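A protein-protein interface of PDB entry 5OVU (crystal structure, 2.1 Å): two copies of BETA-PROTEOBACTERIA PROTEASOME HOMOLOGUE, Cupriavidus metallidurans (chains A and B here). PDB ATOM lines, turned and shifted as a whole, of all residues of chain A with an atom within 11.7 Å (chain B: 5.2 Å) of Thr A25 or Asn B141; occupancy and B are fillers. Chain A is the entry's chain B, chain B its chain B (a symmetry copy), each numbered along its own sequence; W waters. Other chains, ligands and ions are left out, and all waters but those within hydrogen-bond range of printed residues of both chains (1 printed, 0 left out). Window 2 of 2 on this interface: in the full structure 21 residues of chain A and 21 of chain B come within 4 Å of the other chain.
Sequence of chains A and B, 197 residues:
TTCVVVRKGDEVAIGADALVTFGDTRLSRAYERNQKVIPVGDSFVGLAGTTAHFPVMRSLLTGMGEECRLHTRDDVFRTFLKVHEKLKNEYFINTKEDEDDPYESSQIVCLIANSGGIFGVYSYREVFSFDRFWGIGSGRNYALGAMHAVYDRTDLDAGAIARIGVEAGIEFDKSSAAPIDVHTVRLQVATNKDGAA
The side-chain hydroxyl of Thr A25 lies within hydrogen-bond range of the side-chain amide oxygen of Asn B141.
The backbone carbonyl oxygen (O) of Val A20 sits at hydrogen-bond distance from the backbone NH (N) of Leu A27 (3.0 Å). OD1 of Asn B141 is in hydrogen-bond range of NE of Arg B140, at 3.1 Å.
Among the printed residues, pairs that only touch across the chains: Phe A22 with Trp B134, Phe A22 with Arg B140, Thr A25 with Trp B134, Thr A25 with Arg B140, Thr A25 with Leu B144, Arg A26 with Trp B134 and Leu A27 with Trp B134.
Ala A18 touches none of the printed residues of chain B. Of the printed residues of chain B, Phe A22 touches Trp B134 (3.6 Å) and Arg B140 (3.8 Å). Of chain B, only Trp B134, Arg B140, Asn B141 and Leu B144 come within 4 Å of Thr A25. Of the printed residues of chain B, Arg A26 touches Trp B134 (3.4 Å). Printed residues of chain B within 4 Å of Leu A27: Trp B134. Of the printed residues of chain A, Trp B134 touches Phe A22, Thr A25, Arg A26 and Leu A27. Gly B137 touches none of the printed residues of chain A. No residue of chain A comes within 4 Å of Gly B139. Arg B140 touches just these residues of chain A: Phe A22 (3.8 Å) and Thr A25 (3.6 Å). Of chain A, only Thr A25 comes within 4 Å of Asn B141. Tyr B142 touches none of the printed residues of chain A. No residue of chain A comes within 4 Å of Ala B143. No residue of chain A comes within 4 Å of Gly B145. The nearest printed residue of chain B that does not touch Thr A25 is Gly B145 (8.0 Å).
Of the 10 printed residues of chain B, 4 touch a printed residue of chain A. Along chain B the printed residues that touch a printed residue of chain A span positions 134 to 144. Among the printed residues, 8 pairs touch across the chains. Among the printed residues, no Asp or Glu carboxylate lies within 4 Å of a Lys or Arg side-chain nitrogen of the other chain.
No position is printed for both chains.
Water W1 lies within hydrogen-bond range of ND2 of Asn B141 (2.9 Å) and OG1 of Thr A25 (3.4 Å).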
ATOM      1  N   ALA A  18       7.440  -4.888 -19.389  1.00  0.00           N
ATOM      2  CA  ALA A  18       6.240  -5.364 -18.690  1.00  0.00           C
ATOM      3  C   ALA A  18       5.027  -4.430 -18.736  1.00  0.00           C
ATOM      4  O   ALA A  18       3.951  -4.821 -18.285  1.00  0.00           O
ATOM      5  CB  ALA A  18       6.583  -5.670 -17.245  1.00  0.00           C
ATOM      6  N   LEU A  19       5.182  -3.213 -19.258  1.00  0.00           N
ATOM      7  CA  LEU A  19       4.104  -2.222 -19.188  1.00  0.00           C
ATOM      8  C   LEU A  19       2.890  -2.652 -20.006  1.00  0.00           C
ATOM      9  O   LEU A  19       3.011  -2.983 -21.189  1.00  0.00           O
ATOM     10  CB  LEU A  19       4.583  -0.843 -19.659  1.00  0.00           C
ATOM     11  CG  LEU A  19       3.572   0.310 -19.527  1.00  0.00           C
ATOM     12  CD1 LEU A  19       3.155   0.512 -18.076  1.00  0.00           C
ATOM     13  CD2 LEU A  19       4.133   1.599 -20.111  1.00  0.00           C
ATOM     14  N   VAL A  20       1.726  -2.650 -19.359  1.00  0.00           N
ATOM     15  CA  VAL A  20       0.457  -2.911 -20.032  1.00  0.00           C
ATOM     16  C   VAL A  20      -0.553  -1.830 -19.648  1.00  0.00           C
ATOM     17  O   VAL A  20      -0.668  -1.465 -18.475  1.00  0.00           O
ATOM     18  CB  VAL A  20      -0.093  -4.322 -19.725  1.00  0.00           C
ATOM     19  CG1 VAL A  20       0.786  -5.384 -20.370  1.00  0.00           C
ATOM     20  CG2 VAL A  20      -0.223  -4.569 -18.226  1.00  0.00           C
ATOM     21  N   THR A  21      -1.264  -1.308 -20.646  1.00  0.00           N
ATOM     22  CA  THR A  21      -2.195  -0.200 -20.444  1.00  0.00           C
ATOM     23  C   THR A  21      -3.483  -0.397 -21.234  1.00  0.00           C
ATOM     24  O   THR A  21      -3.490  -1.049 -22.276  1.00  0.00           O
ATOM     25  CB  THR A  21      -1.583   1.144 -20.896  1.00  0.00           C
ATOM     26  OG1 THR A  21      -1.421   1.146 -22.320  1.00  0.00           O
ATOM     27  CG2 THR A  21      -0.232   1.381 -20.248  1.00  0.00           C
ATOM     28  N   PHE A  22      -4.570   0.160 -20.709  1.00  0.00           N
ATOM     29  CA  PHE A  22      -5.781   0.386 -21.483  1.00  0.00           C
ATOM     30  C   PHE A  22      -5.758   1.861 -21.871  1.00  0.00           C
ATOM     31  O   PHE A  22      -6.175   2.719 -21.095  1.00  0.00           O
ATOM     32  CB  PHE A  22      -7.037   0.076 -20.661  1.00  0.00           C
ATOM     33  CG  PHE A  22      -7.318  -1.394 -20.493  1.00  0.00           C
ATOM     34  CD1 PHE A  22      -7.489  -2.216 -21.600  1.00  0.00           C
ATOM     35  CD2 PHE A  22      -7.446  -1.950 -19.227  1.00  0.00           C
ATOM     36  CE1 PHE A  22      -7.760  -3.566 -21.445  1.00  0.00           C
ATOM     37  CE2 PHE A  22      -7.720  -3.299 -19.066  1.00  0.00           C
ATOM     38  CZ  PHE A  22      -7.878  -4.107 -20.177  1.00  0.00           C
ATOM     39  N   GLY A  23      -5.236   2.151 -23.058  1.00  0.00           N
ATOM     40  CA  GLY A  23      -5.039   3.531 -23.495  1.00  0.00           C
ATOM     41  C   GLY A  23      -3.930   4.194 -22.703  1.00  0.00           C
ATOM     42  O   GLY A  23      -2.814   3.673 -22.641  1.00  0.00           O
ATOM     43  N   ASP A  24      -4.241   5.333 -22.088  1.00  0.00           N
ATOM     44  CA  ASP A  24      -3.284   6.072 -21.253  1.00  0.00           C
ATOM     45  C   ASP A  24      -3.280   5.623 -19.789  1.00  0.00           C
ATOM     46  O   ASP A  24      -2.409   6.039 -19.025  1.00  0.00           O
ATOM     47  CB  ASP A  24      -3.582   7.576 -21.301  1.00  0.00           C
ATOM     48  CG  ASP A  24      -3.422   8.167 -22.690  1.00  0.00           C
ATOM     49  OD1 ASP A  24      -2.660   7.610 -23.509  1.00  0.00           O
ATOM     50  OD2 ASP A  24      -4.060   9.204 -22.960  1.00  0.00           O
ATOM     51  N   THR A  25      -4.245   4.792 -19.396  1.00  0.00           N
ATOM     52  CA  THR A  25      -4.352   4.327 -18.013  1.00  0.00           C
ATOM     53  C   THR A  25      -3.600   3.010 -17.817  1.00  0.00           C
ATOM     54  O   THR A  25      -3.908   2.009 -18.462  1.00  0.00           O
ATOM     55  CB  THR A  25      -5.826   4.135 -17.602  1.00  0.00           C
ATOM     56  OG1 THR A  25      -6.571   5.317 -17.921  1.00  0.00           O
ATOM     57  CG2 THR A  25      -5.943   3.856 -16.109  1.00  0.00           C
ATOM     58  N   ARG A  26      -2.617   3.018 -16.920  1.00  0.00           N
ATOM     59  CA  ARG A  26      -1.825   1.821 -16.626  1.00  0.00           C
ATOM     60  C   ARG A  26      -2.634   0.752 -15.884  1.00  0.00           C
ATOM     61  O   ARG A  26      -3.451   1.064 -15.012  1.00  0.00           O
ATOM     62  CB  ARG A  26      -0.582   2.183 -15.804  1.00  0.00           C
ATOM     63  CG  ARG A  26       0.201   0.973 -15.315  1.00  0.00           C
ATOM     64  CD  ARG A  26       1.605   1.337 -14.871  1.00  0.00           C
ATOM     65  NE  ARG A  26       2.458   0.153 -14.801  1.00  0.00           N
ATOM     66  CZ  ARG A  26       3.768   0.175 -14.565  1.00  0.00           C
ATOM     67  NH1 ARG A  26       4.405   1.329 -14.367  1.00  0.00           N
ATOM     68  NH2 ARG A  26       4.448  -0.964 -14.527  1.00  0.00           N
ATOM     69  N   LEU A  27      -2.382  -0.503 -16.243  1.00  0.00           N
ATOM     70  CA  LEU A  27      -2.993  -1.661 -15.597  1.00  0.00           C
ATOM     71  C   LEU A  27      -1.921  -2.415 -14.808  1.00  0.00           C
ATOM     72  O   LEU A  27      -0.926  -2.853 -15.382  1.00  0.00           O
ATOM     73  CB  LEU A  27      -3.602  -2.577 -16.663  1.00  0.00           C
ATOM     74  CG  LEU A  27      -4.339  -3.838 -16.203  1.00  0.00           C
ATOM     75  CD1 LEU A  27      -5.652  -3.482 -15.525  1.00  0.00           C
ATOM     76  CD2 LEU A  27      -4.581  -4.764 -17.384  1.00  0.00           C
ATOM     77  N   SER A  28      -2.126  -2.554 -13.498  1.00  0.00           N
ATOM     78  CA  SER A  28      -1.212  -3.307 -12.635  1.00  0.00           C
ATOM     79  C   SER A  28      -1.515  -4.796 -12.731  1.00  0.00           C
ATOM     80  O   SER A  28      -2.681  -5.195 -12.733  1.00  0.00           O
ATOM     81  CB  SER A  28      -1.361  -2.860 -11.178  1.00  0.00           C
ATOM     82  OG  SER A  28      -1.321  -1.450 -11.077  1.00  0.00           O
ATOM     83  N   ARG A  29      -0.466  -5.613 -12.794  1.00  0.00           N
ATOM     84  CA  ARG A  29      -0.620  -7.057 -12.975  1.00  0.00           C
ATOM     85  C   ARG A  29       0.178  -7.871 -11.963  1.00  0.00           C
ATOM     86  O   ARG A  29       1.022  -7.335 -11.239  1.00  0.00           O
ATOM     87  CB  ARG A  29      -0.239  -7.446 -14.410  1.00  0.00           C
ATOM     88  CG  ARG A  29      -1.400  -7.356 -15.388  1.00  0.00           C
ATOM     89  CD  ARG A  29      -2.287  -8.591 -15.299  1.00  0.00           C
ATOM     90  NE  ARG A  29      -3.643  -8.358 -15.799  1.00  0.00           N
ATOM     91  CZ  ARG A  29      -4.640  -7.816 -15.095  1.00  0.00           C
ATOM     92  NH1 ARG A  29      -4.458  -7.413 -13.840  1.00  0.00           N
ATOM     93  NH2 ARG A  29      -5.835  -7.667 -15.655  1.00  0.00           N
ATOM     94  N   LYS A  36       2.857  -9.960 -22.249  1.00  0.00           N
ATOM     95  CA  LYS A  36       3.069  -9.829 -23.699  1.00  0.00           C
ATOM     96  C   LYS A  36       4.028 -10.853 -24.327  1.00  0.00           C
ATOM     97  O   LYS A  36       4.153 -10.895 -25.552  1.00  0.00           O
ATOM     98  CB  LYS A  36       3.508  -8.402 -24.061  1.00  0.00           C
ATOM     99  CG  LYS A  36       4.917  -8.018 -23.645  1.00  0.00           C
ATOM    100  CD  LYS A  36       5.161  -6.530 -23.851  1.00  0.00           C
ATOM    101  CE  LYS A  36       4.494  -5.692 -22.769  1.00  0.00           C
ATOM    102  NZ  LYS A  36       4.767  -4.234 -22.921  1.00  0.00           N
ATOM    103  N   THR A  50      -1.758  -3.050 -28.828  1.00  0.00           N
ATOM    104  CA  THR A  50      -2.481  -2.738 -27.591  1.00  0.00           C
ATOM    105  C   THR A  50      -2.785  -3.964 -26.721  1.00  0.00           C
ATOM    106  O   THR A  50      -3.053  -5.055 -27.233  1.00  0.00           O
ATOM    107  CB  THR A  50      -3.808  -2.002 -27.895  1.00  0.00           C
ATOM    108  OG1 THR A  50      -4.392  -1.530 -26.676  1.00  0.00           O
ATOM    109  CG2 THR A  50      -4.807  -2.919 -28.608  1.00  0.00           C
ATOM    110  N   THR A  51      -2.756  -3.761 -25.403  1.00  0.00           N
ATOM    111  CA  THR A  51      -3.087  -4.810 -24.429  1.00  0.00           C
ATOM    112  C   THR A  51      -4.493  -5.374 -24.638  1.00  0.00           C
ATOM    113  O   THR A  51      -4.731  -6.559 -24.388  1.00  0.00           O
ATOM    114  CB  THR A  51      -2.997  -4.279 -22.980  1.00  0.00           C
ATOM    115  OG1 THR A  51      -1.704  -3.708 -22.758  1.00  0.00           O
ATOM    116  CG2 THR A  51      -3.234  -5.398 -21.965  1.00  0.00           C
ATOM    117  N   ALA A  52      -5.411  -4.524 -25.097  1.00  0.00           N
ATOM    118  CA  ALA A  52      -6.799  -4.916 -25.325  1.00  0.00           C
ATOM    119  C   ALA A  52      -6.965  -6.124 -26.256  1.00  0.00           C
ATOM    120  O   ALA A  52      -7.947  -6.851 -26.136  1.00  0.00           O
ATOM    121  CB  ALA A  52      -7.600  -3.731 -25.853  1.00  0.00           C
ATOM    122  N   LYS A 174       8.533   6.320 -22.535  1.00  0.00           N
ATOM    123  CA  LYS A 174       7.527   6.380 -21.466  1.00  0.00           C
ATOM    124  C   LYS A 174       6.534   5.212 -21.520  1.00  0.00           C
ATOM    125  O   LYS A 174       5.964   4.837 -20.496  1.00  0.00           O
ATOM    126  CB  LYS A 174       6.776   7.721 -21.480  1.00  0.00           C
ATOM    127  CG  LYS A 174       5.954   8.000 -22.733  1.00  0.00           C
ATOM    128  CD  LYS A 174       4.961   9.134 -22.521  1.00  0.00           C
ATOM    129  CE  LYS A 174       5.658  10.464 -22.288  1.00  0.00           C
ATOM    130  NZ  LYS A 174       4.687  11.594 -22.282  1.00  0.00           N
ATOM    131  N   SER A 175       6.337   4.644 -22.711  1.00  0.00           N
ATOM    132  CA  SER A 175       5.475   3.469 -22.892  1.00  0.00           C
ATOM    133  C   SER A 175       6.205   2.128 -22.723  1.00  0.00           C
ATOM    134  O   SER A 175       5.697   1.090 -23.148  1.00  0.00           O
ATOM    135  CB  SER A 175       4.794   3.526 -24.266  1.00  0.00           C
ATOM    136  OG  SER A 175       3.938   4.652 -24.366  1.00  0.00           O
ATOM    137  N   ALA A 177       8.331  -0.123 -19.532  1.00  0.00           N
ATOM    138  CA  ALA A 177       8.638  -0.156 -18.095  1.00  0.00           C
ATOM    139  C   ALA A 177       9.165  -1.509 -17.606  1.00  0.00           C
ATOM    140  O   ALA A 177       8.808  -2.562 -18.134  1.00  0.00           O
ATOM    141  CB  ALA A 177       7.411   0.243 -17.289  1.00  0.00           C
ATOM    142  N   TRP B 134     -11.124  -2.553 -10.872  1.00  0.00           N
ATOM    143  CA  TRP B 134     -11.041  -1.762 -12.100  1.00  0.00           C
ATOM    144  C   TRP B 134     -12.310  -0.910 -12.254  1.00  0.00           C
ATOM    145  O   TRP B 134     -13.285  -1.109 -11.528  1.00  0.00           O
ATOM    146  CB  TRP B 134     -10.831  -2.654 -13.331  1.00  0.00           C
ATOM    147  CG  TRP B 134     -10.285  -1.896 -14.505  1.00  0.00           C
ATOM    148  CD1 TRP B 134     -10.911  -1.657 -15.697  1.00  0.00           C
ATOM    149  CD2 TRP B 134      -9.016  -1.237 -14.580  1.00  0.00           C
ATOM    150  NE1 TRP B 134     -10.102  -0.903 -16.513  1.00  0.00           N
ATOM    151  CE2 TRP B 134      -8.933  -0.631 -15.852  1.00  0.00           C
ATOM    152  CE3 TRP B 134      -7.937  -1.104 -13.697  1.00  0.00           C
ATOM    153  CZ2 TRP B 134      -7.813   0.097 -16.264  1.00  0.00           C
ATOM    154  CZ3 TRP B 134      -6.824  -0.382 -14.106  1.00  0.00           C
ATOM    155  CH2 TRP B 134      -6.771   0.207 -15.380  1.00  0.00           C
ATOM    156  N   GLY B 137     -15.863   4.078 -17.889  1.00  0.00           N
ATOM    157  CA  GLY B 137     -16.716   5.244 -18.096  1.00  0.00           C
ATOM    158  C   GLY B 137     -15.959   6.540 -17.885  1.00  0.00           C
ATOM    159  O   GLY B 137     -14.776   6.533 -17.538  1.00  0.00           O
ATOM    160  N   SER B 138     -16.659   7.654 -18.066  1.00  0.00           N
ATOM    161  CA  SER B 138     -16.044   8.984 -18.035  1.00  0.00           C
ATOM    162  C   SER B 138     -15.450   9.389 -16.681  1.00  0.00           C
ATOM    163  O   SER B 138     -14.551  10.226 -16.633  1.00  0.00           O
ATOM    164  CB  SER B 138     -17.063  10.041 -18.477  1.00  0.00           C
ATOM    165  OG  SER B 138     -18.267   9.932 -17.736  1.00  0.00           O
ATOM    166  N   GLY B 139     -15.945   8.812 -15.587  1.00  0.00           N
ATOM    167  CA  GLY B 139     -15.421   9.134 -14.260  1.00  0.00           C
ATOM    168  C   GLY B 139     -14.468   8.107 -13.668  1.00  0.00           C
ATOM    169  O   GLY B 139     -14.160   8.177 -12.480  1.00  0.00           O
ATOM    170  N   ARG B 140     -13.979   7.171 -14.484  1.00  0.00           N
ATOM    171  CA  ARG B 140     -13.230   6.018 -13.966  1.00  0.00           C
ATOM    172  C   ARG B 140     -11.828   6.357 -13.453  1.00  0.00           C
ATOM    173  O   ARG B 140     -11.344   5.709 -12.526  1.00  0.00           O
ATOM    174  CB  ARG B 140     -13.166   4.882 -15.001  1.00  0.00           C
ATOM    175  CG  ARG B 140     -12.187   5.069 -16.156  1.00  0.00           C
ATOM    176  CD  ARG B 140     -10.840   4.402 -15.889  1.00  0.00           C
ATOM    177  NE  ARG B 140     -10.028   4.268 -17.100  1.00  0.00           N
ATOM    178  CZ  ARG B 140     -10.134   3.281 -17.992  1.00  0.00           C
ATOM    179  NH1 ARG B 140     -11.028   2.308 -17.845  1.00  0.00           N
ATOM    180  NH2 ARG B 140      -9.337   3.268 -19.054  1.00  0.00           N
ATOM    181  N   ASN B 141     -11.182   7.360 -14.044  1.00  0.00           N
ATOM    182  CA  ASN B 141      -9.849   7.769 -13.586  1.00  0.00           C
ATOM    183  C   ASN B 141      -9.868   8.298 -12.151  1.00  0.00           C
ATOM    184  O   ASN B 141      -8.971   7.996 -11.360  1.00  0.00           O
ATOM    185  CB  ASN B 141      -9.232   8.801 -14.534  1.00  0.00           C
ATOM    186  CG  ASN B 141      -8.832   8.204 -15.874  1.00  0.00           C
ATOM    187  OD1 ASN B 141      -8.960   6.997 -16.103  1.00  0.00           O
ATOM    188  ND2 ASN B 141      -8.339   9.049 -16.766  1.00  0.00           N
ATOM    189  N   TYR B 142     -10.900   9.068 -11.819  1.00  0.00           N
ATOM    190  CA  TYR B 142     -11.097   9.542 -10.449  1.00  0.00           C
ATOM    191  C   TYR B 142     -11.344   8.352  -9.519  1.00  0.00           C
ATOM    192  O   TYR B 142     -10.804   8.292  -8.411  1.00  0.00           O
ATOM    193  CB  TYR B 142     -12.278  10.514 -10.362  1.00  0.00           C
ATOM    194  CG  TYR B 142     -12.245  11.684 -11.334  1.00  0.00           C
ATOM    195  CD1 TYR B 142     -11.425  12.789 -11.108  1.00  0.00           C
ATOM    196  CD2 TYR B 142     -13.063  11.697 -12.466  1.00  0.00           C
ATOM    197  CE1 TYR B 142     -11.404  13.860 -11.989  1.00  0.00           C
ATOM    198  CE2 TYR B 142     -13.050  12.764 -13.355  1.00  0.00           C
ATOM    199  CZ  TYR B 142     -12.222  13.846 -13.112  1.00  0.00           C
ATOM    200  OH  TYR B 142     -12.213  14.903 -13.991  1.00  0.00           O
ATOM    201  N   ALA B 143     -12.160   7.406  -9.985  1.00  0.00           N
ATOM    202  CA  ALA B 143     -12.510   6.213  -9.213  1.00  0.00           C
ATOM    203  C   ALA B 143     -11.301   5.325  -8.929  1.00  0.00           C
ATOM    204  O   ALA B 143     -11.136   4.839  -7.810  1.00  0.00           O
ATOM    205  CB  ALA B 143     -13.586   5.416  -9.936  1.00  0.00           C
ATOM    206  N   LEU B 144     -10.459   5.120  -9.941  1.00  0.00           N
ATOM    207  CA  LEU B 144      -9.249   4.300  -9.791  1.00  0.00           C
ATOM    208  C   LEU B 144      -8.292   4.868  -8.741  1.00  0.00           C
ATOM    209  O   LEU B 144      -7.758   4.128  -7.912  1.00  0.00           O
ATOM    210  CB  LEU B 144      -8.527   4.144 -11.131  1.00  0.00           C
ATOM    211  CG  LEU B 144      -9.202   3.250 -12.177  1.00  0.00           C
ATOM    212  CD1 LEU B 144      -8.470   3.357 -13.507  1.00  0.00           C
ATOM    213  CD2 LEU B 144      -9.270   1.803 -11.715  1.00  0.00           C
ATOM    214  N   GLY B 145      -8.084   6.182  -8.784  1.00  0.00           N
ATOM    215  CA  GLY B 145      -7.261   6.872  -7.793  1.00  0.00           C
ATOM    216  C   GLY B 145      -7.786   6.737  -6.372  1.00  0.00           C
ATOM    217  O   GLY B 145      -7.007   6.560  -5.433  1.00  0.00           O
HETATM  218  O   HOH W   1      -7.180   8.374 -19.379  1.00  0.00           O
